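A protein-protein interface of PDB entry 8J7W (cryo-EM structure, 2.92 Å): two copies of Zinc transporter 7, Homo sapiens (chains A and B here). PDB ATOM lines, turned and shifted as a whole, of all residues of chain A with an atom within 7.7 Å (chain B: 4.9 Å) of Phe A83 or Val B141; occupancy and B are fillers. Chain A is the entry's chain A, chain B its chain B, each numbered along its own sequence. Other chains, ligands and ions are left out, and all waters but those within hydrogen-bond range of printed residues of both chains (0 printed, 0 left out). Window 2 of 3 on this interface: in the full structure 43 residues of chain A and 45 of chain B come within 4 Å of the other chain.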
ATOM      1  N   GLU A  66       7.946 -30.449 -30.605  1.00  0.00           N
ATOM      2  CA  GLU A  66       7.558 -30.793 -29.246  1.00  0.00           C
ATOM      3  C   GLU A  66       6.047 -30.738 -29.052  1.00  0.00           C
ATOM      4  O   GLU A  66       5.527 -31.433 -28.180  1.00  0.00           O
ATOM      5  CB  GLU A  66       8.332 -29.920 -28.239  1.00  0.00           C
ATOM      6  CG  GLU A  66       8.056 -28.408 -28.167  1.00  0.00           C
ATOM      7  CD  GLU A  66       6.667 -28.053 -27.709  1.00  0.00           C
ATOM      8  OE1 GLU A  66       6.206 -28.679 -26.732  1.00  0.00           O
ATOM      9  OE2 GLU A  66       6.051 -27.151 -28.313  1.00  0.00           O
ATOM     10  N   LEU A  67       5.355 -29.969 -29.899  1.00  0.00           N
ATOM     11  CA  LEU A  67       3.870 -29.967 -29.855  1.00  0.00           C
ATOM     12  C   LEU A  67       3.400 -31.335 -30.352  1.00  0.00           C
ATOM     13  O   LEU A  67       2.480 -31.905 -29.737  1.00  0.00           O
ATOM     14  CB  LEU A  67       3.347 -28.844 -30.755  1.00  0.00           C
ATOM     15  CG  LEU A  67       1.870 -28.937 -31.132  1.00  0.00           C
ATOM     16  CD1 LEU A  67       0.988 -28.474 -29.983  1.00  0.00           C
ATOM     17  CD2 LEU A  67       1.580 -28.130 -32.387  1.00  0.00           C
ATOM     18  N   GLY A  77       2.344 -32.300 -18.387  1.00  0.00           N
ATOM     19  CA  GLY A  77       2.827 -30.928 -18.138  1.00  0.00           C
ATOM     20  C   GLY A  77       3.525 -30.308 -19.339  1.00  0.00           C
ATOM     21  O   GLY A  77       3.896 -29.122 -19.239  1.00  0.00           O
ATOM     22  N   LEU A  78       3.700 -31.052 -20.438  1.00  0.00           N
ATOM     23  CA  LEU A  78       4.492 -30.496 -21.574  1.00  0.00           C
ATOM     24  C   LEU A  78       3.669 -29.466 -22.355  1.00  0.00           C
ATOM     25  O   LEU A  78       4.275 -28.504 -22.859  1.00  0.00           O
ATOM     26  CB  LEU A  78       5.020 -31.614 -22.484  1.00  0.00           C
ATOM     27  CG  LEU A  78       4.107 -32.813 -22.715  1.00  0.00           C
ATOM     28  CD1 LEU A  78       2.958 -32.454 -23.642  1.00  0.00           C
ATOM     29  CD2 LEU A  78       4.904 -33.972 -23.295  1.00  0.00           C
ATOM     30  N   ILE A  79       2.354 -29.656 -22.472  1.00  0.00           N
ATOM     31  CA  ILE A  79       1.565 -28.610 -23.130  1.00  0.00           C
ATOM     32  C   ILE A  79       1.859 -27.250 -22.499  1.00  0.00           C
ATOM     33  O   ILE A  79       2.005 -26.234 -23.201  1.00  0.00           O
ATOM     34  CB  ILE A  79       0.061 -28.952 -23.108  1.00  0.00           C
ATOM     35  CG1 ILE A  79      -0.209 -30.227 -23.920  1.00  0.00           C
ATOM     36  CG2 ILE A  79      -0.773 -27.793 -23.628  1.00  0.00           C
ATOM     37  CD1 ILE A  79       0.198 -30.119 -25.378  1.00  0.00           C
ATOM     38  N   SER A  80       1.979 -27.213 -21.168  1.00  0.00           N
ATOM     39  CA  SER A  80       2.392 -25.988 -20.492  1.00  0.00           C
ATOM     40  C   SER A  80       3.790 -25.567 -20.922  1.00  0.00           C
ATOM     41  O   SER A  80       4.041 -24.380 -21.158  1.00  0.00           O
ATOM     42  CB  SER A  80       2.335 -26.179 -18.978  1.00  0.00           C
ATOM     43  OG  SER A  80       3.119 -25.199 -18.323  1.00  0.00           O
ATOM     44  N   ASP A  81       4.716 -26.528 -21.023  1.00  0.00           N
ATOM     45  CA  ASP A  81       6.067 -26.194 -21.481  1.00  0.00           C
ATOM     46  C   ASP A  81       6.054 -25.654 -22.911  1.00  0.00           C
ATOM     47  O   ASP A  81       6.774 -24.698 -23.228  1.00  0.00           O
ATOM     48  CB  ASP A  81       7.004 -27.401 -21.371  1.00  0.00           C
ATOM     49  CG  ASP A  81       6.869 -28.133 -20.048  1.00  0.00           C
ATOM     50  OD1 ASP A  81       6.760 -27.456 -19.007  1.00  0.00           O
ATOM     51  OD2 ASP A  81       6.930 -29.379 -20.036  1.00  0.00           O
ATOM     52  N   SER A  82       5.241 -26.261 -23.784  1.00  0.00           N
ATOM     53  CA  SER A  82       5.088 -25.778 -25.152  1.00  0.00           C
ATOM     54  C   SER A  82       4.633 -24.332 -25.169  1.00  0.00           C
ATOM     55  O   SER A  82       5.210 -23.493 -25.869  1.00  0.00           O
ATOM     56  CB  SER A  82       4.069 -26.638 -25.899  1.00  0.00           C
ATOM     57  OG  SER A  82       2.784 -26.533 -25.314  1.00  0.00           O
ATOM     58  N   PHE A  83       3.603 -24.020 -24.387  1.00  0.00           N
ATOM     59  CA  PHE A  83       3.083 -22.659 -24.386  1.00  0.00           C
ATOM     60  C   PHE A  83       4.105 -21.686 -23.805  1.00  0.00           C
ATOM     61  O   PHE A  83       4.225 -20.548 -24.276  1.00  0.00           O
ATOM     62  CB  PHE A  83       1.762 -22.617 -23.622  1.00  0.00           C
ATOM     63  CG  PHE A  83       0.612 -23.257 -24.362  1.00  0.00           C
ATOM     64  CD1 PHE A  83       0.794 -23.803 -25.625  1.00  0.00           C
ATOM     65  CD2 PHE A  83      -0.644 -23.334 -23.786  1.00  0.00           C
ATOM     66  CE1 PHE A  83      -0.252 -24.397 -26.301  1.00  0.00           C
ATOM     67  CE2 PHE A  83      -1.695 -23.929 -24.457  1.00  0.00           C
ATOM     68  CZ  PHE A  83      -1.497 -24.461 -25.718  1.00  0.00           C
ATOM     69  N   HIS A  84       4.881 -22.128 -22.812  1.00  0.00           N
ATOM     70  CA  HIS A  84       5.901 -21.249 -22.248  1.00  0.00           C
ATOM     71  C   HIS A  84       7.013 -20.946 -23.248  1.00  0.00           C
ATOM     72  O   HIS A  84       7.498 -19.809 -23.304  1.00  0.00           O
ATOM     73  CB  HIS A  84       6.476 -21.848 -20.961  1.00  0.00           C
ATOM     74  CG  HIS A  84       7.652 -21.095 -20.414  1.00  0.00           C
ATOM     75  ND1 HIS A  84       7.572 -20.324 -19.274  1.00  0.00           N
ATOM     76  CD2 HIS A  84       8.947 -21.041 -20.810  1.00  0.00           C
ATOM     77  CE1 HIS A  84       8.754 -19.796 -19.015  1.00  0.00           C
ATOM     78  NE2 HIS A  84       9.607 -20.215 -19.932  1.00  0.00           N
ATOM     79  N   MET A  85       7.451 -21.922 -24.046  1.00  0.00           N
ATOM     80  CA  MET A  85       8.496 -21.533 -24.990  1.00  0.00           C
ATOM     81  C   MET A  85       7.898 -20.863 -26.225  1.00  0.00           C
ATOM     82  O   MET A  85       8.622 -20.197 -26.971  1.00  0.00           O
ATOM     83  CB  MET A  85       9.420 -22.699 -25.363  1.00  0.00           C
ATOM     84  CG  MET A  85       8.841 -24.080 -25.421  1.00  0.00           C
ATOM     85  SD  MET A  85       7.954 -24.303 -26.961  1.00  0.00           S
ATOM     86  CE  MET A  85       9.358 -24.556 -28.042  1.00  0.00           C
ATOM     87  N   PHE A  86       6.578 -20.964 -26.425  1.00  0.00           N
ATOM     88  CA  PHE A  86       5.914 -20.010 -27.316  1.00  0.00           C
ATOM     89  C   PHE A  86       6.039 -18.586 -26.783  1.00  0.00           C
ATOM     90  O   PHE A  86       6.260 -17.644 -27.552  1.00  0.00           O
ATOM     91  CB  PHE A  86       4.437 -20.362 -27.517  1.00  0.00           C
ATOM     92  CG  PHE A  86       4.196 -21.505 -28.461  1.00  0.00           C
ATOM     93  CD1 PHE A  86       4.703 -21.467 -29.749  1.00  0.00           C
ATOM     94  CD2 PHE A  86       3.410 -22.582 -28.088  1.00  0.00           C
ATOM     95  CE1 PHE A  86       4.473 -22.505 -30.631  1.00  0.00           C
ATOM     96  CE2 PHE A  86       3.176 -23.625 -28.965  1.00  0.00           C
ATOM     97  CZ  PHE A  86       3.707 -23.584 -30.240  1.00  0.00           C
ATOM     98  N   PHE A  87       5.883 -18.411 -25.469  1.00  0.00           N
ATOM     99  CA  PHE A  87       6.127 -17.104 -24.852  1.00  0.00           C
ATOM    100  C   PHE A  87       7.566 -16.650 -25.084  1.00  0.00           C
ATOM    101  O   PHE A  87       7.831 -15.471 -25.355  1.00  0.00           O
ATOM    102  CB  PHE A  87       5.838 -17.167 -23.352  1.00  0.00           C
ATOM    103  CG  PHE A  87       4.402 -16.950 -22.992  1.00  0.00           C
ATOM    104  CD1 PHE A  87       3.409 -17.752 -23.523  1.00  0.00           C
ATOM    105  CD2 PHE A  87       4.048 -15.967 -22.085  1.00  0.00           C
ATOM    106  CE1 PHE A  87       2.093 -17.566 -23.182  1.00  0.00           C
ATOM    107  CE2 PHE A  87       2.732 -15.777 -21.740  1.00  0.00           C
ATOM    108  CZ  PHE A  87       1.756 -16.582 -22.288  1.00  0.00           C
ATOM    109  N   ASP A  88       8.512 -17.581 -24.949  1.00  0.00           N
ATOM    110  CA  ASP A  88       9.917 -17.258 -25.187  1.00  0.00           C
ATOM    111  C   ASP A  88      10.151 -16.833 -26.636  1.00  0.00           C
ATOM    112  O   ASP A  88      10.898 -15.881 -26.906  1.00  0.00           O
ATOM    113  CB  ASP A  88      10.794 -18.458 -24.831  1.00  0.00           C
ATOM    114  CG  ASP A  88      11.128 -18.517 -23.355  1.00  0.00           C
ATOM    115  OD1 ASP A  88      10.335 -17.994 -22.543  1.00  0.00           O
ATOM    116  OD2 ASP A  88      12.182 -19.087 -23.004  1.00  0.00           O
ATOM    117  N   SER A  89       9.521 -17.534 -27.582  1.00  0.00           N
ATOM    118  CA  SER A  89       9.601 -17.143 -28.985  1.00  0.00           C
ATOM    119  C   SER A  89       8.975 -15.774 -29.212  1.00  0.00           C
ATOM    120  O   SER A  89       9.446 -14.999 -30.051  1.00  0.00           O
ATOM    121  CB  SER A  89       8.922 -18.195 -29.861  1.00  0.00           C
ATOM    122  OG  SER A  89       8.349 -17.604 -31.014  1.00  0.00           O
ATOM    123  N   THR A  90       7.904 -15.462 -28.478  1.00  0.00           N
ATOM    124  CA  THR A  90       7.304 -14.133 -28.565  1.00  0.00           C
ATOM    125  C   THR A  90       8.271 -13.060 -28.079  1.00  0.00           C
ATOM    126  O   THR A  90       8.349 -11.975 -28.663  1.00  0.00           O
ATOM    127  CB  THR A  90       6.005 -14.088 -27.759  1.00  0.00           C
ATOM    128  OG1 THR A  90       5.200 -15.228 -28.082  1.00  0.00           O
ATOM    129  CG2 THR A  90       5.227 -12.819 -28.072  1.00  0.00           C
ATOM    130  N   PHE A 128       9.297  -8.954 -18.498  1.00  0.00           N
ATOM    131  CA  PHE A 128       8.933 -10.331 -18.814  1.00  0.00           C
ATOM    132  C   PHE A 128       9.783 -11.318 -18.027  1.00  0.00           C
ATOM    133  O   PHE A 128       9.311 -12.399 -17.662  1.00  0.00           O
ATOM    134  CB  PHE A 128       9.076 -10.576 -20.315  1.00  0.00           C
ATOM    135  CG  PHE A 128       8.351 -11.799 -20.804  1.00  0.00           C
ATOM    136  CD1 PHE A 128       7.278 -12.316 -20.098  1.00  0.00           C
ATOM    137  CD2 PHE A 128       8.744 -12.430 -21.973  1.00  0.00           C
ATOM    138  CE1 PHE A 128       6.611 -13.440 -20.547  1.00  0.00           C
ATOM    139  CE2 PHE A 128       8.081 -13.554 -22.427  1.00  0.00           C
ATOM    140  CZ  PHE A 128       7.013 -14.059 -21.712  1.00  0.00           C
ATOM    141  N   PHE B 137      -4.445 -16.960 -20.887  1.00  0.00           N
ATOM    142  CA  PHE B 137      -4.789 -17.526 -22.190  1.00  0.00           C
ATOM    143  C   PHE B 137      -4.147 -18.897 -22.362  1.00  0.00           C
ATOM    144  O   PHE B 137      -4.795 -19.855 -22.804  1.00  0.00           O
ATOM    145  CB  PHE B 137      -4.338 -16.547 -23.288  1.00  0.00           C
ATOM    146  CG  PHE B 137      -4.639 -16.986 -24.707  1.00  0.00           C
ATOM    147  CD1 PHE B 137      -3.914 -17.996 -25.328  1.00  0.00           C
ATOM    148  CD2 PHE B 137      -5.589 -16.311 -25.453  1.00  0.00           C
ATOM    149  CE1 PHE B 137      -4.181 -18.368 -26.629  1.00  0.00           C
ATOM    150  CE2 PHE B 137      -5.854 -16.675 -26.761  1.00  0.00           C
ATOM    151  CZ  PHE B 137      -5.152 -17.705 -27.347  1.00  0.00           C
ATOM    152  N   SER B 138      -2.860 -18.996 -22.023  1.00  0.00           N
ATOM    153  CA  SER B 138      -2.153 -20.272 -22.097  1.00  0.00           C
ATOM    154  C   SER B 138      -2.815 -21.324 -21.216  1.00  0.00           C
ATOM    155  O   SER B 138      -3.087 -22.449 -21.658  1.00  0.00           O
ATOM    156  CB  SER B 138      -0.695 -20.073 -21.685  1.00  0.00           C
ATOM    157  OG  SER B 138      -0.064 -21.314 -21.436  1.00  0.00           O
ATOM    158  N   GLU B 139      -3.093 -20.964 -19.961  1.00  0.00           N
ATOM    159  CA  GLU B 139      -3.709 -21.919 -19.049  1.00  0.00           C
ATOM    160  C   GLU B 139      -5.136 -22.253 -19.474  1.00  0.00           C
ATOM    161  O   GLU B 139      -5.598 -23.375 -19.247  1.00  0.00           O
ATOM    162  CB  GLU B 139      -3.675 -21.378 -17.618  1.00  0.00           C
ATOM    163  CG  GLU B 139      -4.174 -22.349 -16.552  1.00  0.00           C
ATOM    164  CD  GLU B 139      -3.113 -23.336 -16.089  1.00  0.00           C
ATOM    165  OE1 GLU B 139      -2.366 -23.871 -16.935  1.00  0.00           O
ATOM    166  OE2 GLU B 139      -3.028 -23.580 -14.866  1.00  0.00           O
ATOM    167  N   GLY B 140      -5.835 -21.314 -20.113  1.00  0.00           N
ATOM    168  CA  GLY B 140      -7.165 -21.605 -20.619  1.00  0.00           C
ATOM    169  C   GLY B 140      -7.156 -22.597 -21.764  1.00  0.00           C
ATOM    170  O   GLY B 140      -8.007 -23.486 -21.830  1.00  0.00           O
ATOM    171  N   VAL B 141      -6.200 -22.458 -22.685  1.00  0.00           N
ATOM    172  CA  VAL B 141      -6.083 -23.443 -23.758  1.00  0.00           C
ATOM    173  C   VAL B 141      -5.691 -24.801 -23.188  1.00  0.00           C
ATOM    174  O   VAL B 141      -6.188 -25.847 -23.631  1.00  0.00           O
ATOM    175  CB  VAL B 141      -5.093 -22.962 -24.834  1.00  0.00           C
ATOM    176  CG1 VAL B 141      -4.999 -23.979 -25.959  1.00  0.00           C
ATOM    177  CG2 VAL B 141      -5.529 -21.617 -25.388  1.00  0.00           C
ATOM    178  N   GLU B 142      -4.810 -24.808 -22.180  1.00  0.00           N
ATOM    179  CA  GLU B 142      -4.439 -26.068 -21.537  1.00  0.00           C
ATOM    180  C   GLU B 142      -5.645 -26.722 -20.866  1.00  0.00           C
ATOM    181  O   GLU B 142      -5.819 -27.945 -20.942  1.00  0.00           O
ATOM    182  CB  GLU B 142      -3.304 -25.826 -20.535  1.00  0.00           C
ATOM    183  CG  GLU B 142      -3.056 -26.947 -19.521  1.00  0.00           C
ATOM    184  CD  GLU B 142      -3.868 -26.800 -18.246  1.00  0.00           C
ATOM    185  OE1 GLU B 142      -4.484 -25.731 -18.052  1.00  0.00           O
ATOM    186  OE2 GLU B 142      -3.892 -27.753 -17.439  1.00  0.00           O
ATOM    187  N   ARG B 143      -6.501 -25.908 -20.239  1.00  0.00           N
ATOM    188  CA  ARG B 143      -7.706 -26.453 -19.552  1.00  0.00           C
ATOM    189  C   ARG B 143      -8.725 -26.927 -20.594  1.00  0.00           C
ATOM    190  O   ARG B 143      -9.422 -27.919 -20.321  1.00  0.00           O
ATOM    191  CB  ARG B 143      -8.306 -25.416 -18.597  1.00  0.00           C
ATOM    192  CG  ARG B 143      -7.524 -25.268 -17.302  1.00  0.00           C
ATOM    193  CD  ARG B 143      -8.374 -24.896 -16.103  1.00  0.00           C
ATOM    194  NE  ARG B 143      -7.751 -25.369 -14.876  1.00  0.00           N
ATOM    195  CZ  ARG B 143      -8.245 -25.180 -13.659  1.00  0.00           C
ATOM    196  NH1 ARG B 143      -9.053 -24.162 -13.427  1.00  0.00           N
ATOM    197  NH2 ARG B 143      -7.922 -26.003 -12.677  1.00  0.00           N
ATOM    198  N   ALA B 144      -8.823 -26.238 -21.732  1.00  0.00           N
ATOM    199  CA  ALA B 144      -9.716 -26.676 -22.798  1.00  0.00           C
ATOM    200  C   ALA B 144      -9.238 -27.974 -23.430  1.00  0.00           C
ATOM    201  O   ALA B 144     -10.056 -28.756 -23.928  1.00  0.00           O
ATOM    202  CB  ALA B 144      -9.846 -25.586 -23.861  1.00  0.00           C
ATOM    203  N   LEU B 145      -7.923 -28.200 -23.389  1.00  0.00           N
ATOM    204  CA  LEU B 145      -7.387 -29.491 -23.883  1.00  0.00           C
ATOM    205  C   LEU B 145      -7.967 -30.589 -22.989  1.00  0.00           C
ATOM    206  O   LEU B 145      -8.749 -31.411 -23.502  1.00  0.00           O
ATOM    207  CB  LEU B 145      -5.860 -29.448 -23.802  1.00  0.00           C
ATOM    208  CG  LEU B 145      -5.147 -30.751 -24.150  1.00  0.00           C
ATOM    209  CD1 LEU B 145      -5.112 -30.964 -25.656  1.00  0.00           C
ATOM    210  CD2 LEU B 145      -3.739 -30.754 -23.580  1.00  0.00           C
ATOM    211  N   ILE B 286     -10.196 -17.366 -22.163  1.00  0.00           N
ATOM    212  CA  ILE B 286      -9.719 -16.694 -23.381  1.00  0.00           C
ATOM    213  C   ILE B 286     -10.503 -15.413 -23.658  1.00  0.00           C
ATOM    214  O   ILE B 286      -9.926 -14.407 -24.094  1.00  0.00           O
ATOM    215  CB  ILE B 286      -9.680 -17.619 -24.627  1.00  0.00           C
ATOM    216  CG1 ILE B 286      -8.898 -18.942 -24.459  1.00  0.00           C
ATOM    217  CG2 ILE B 286      -9.171 -16.872 -25.861  1.00  0.00           C
ATOM    218  CD1 ILE B 286      -9.451 -20.030 -23.708  1.00  0.00           C
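Among the printed residues, pairs that only touch across the chains: Ile A79 with Leu B145 (3.6 Å), Phe A83 with Ser B138 (3.1 Å), Phe A83 with Val B141 (3.5 Å) and Phe A83 with Glu B142 (3.96 Å).
Glu A66 touches none of the printed residues of chain B.
Of the printed residues of chain B, Ile A79 touches Leu B145 (3.6 Å).
Of chain B, only Ser B138 (3.1 Å), Val B141 (3.5 Å) and Glu B142 (3.96 Å) come within 4 Å of Phe A83.
No residue of chain A comes within 4 Å of Gly B140.
Of the printed residues of chain A, Glu B142 touches Phe A83.
Ala B144 touches none of the printed residues of chain A.
The nearest residue of chain A that does not touch Val B141 is Ile A79 (5.8 Å).
The nearest printed residue of chain A that does not touch Ser B138 is Phe A87 (4.04 Å).
Printed residues of chain A that touch a printed residue of chain B: Ile A79 and Phe A83.
Among the printed residues, no Asp or Glu carboxylate lies within 4 Å of a Lys or Arg side-chain nitrogen of the other chain.
No position is printed for both chains.
Of the 4 pairs that touch across the chains among the printed residues, none has its exchanged pair printed and touching as well.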
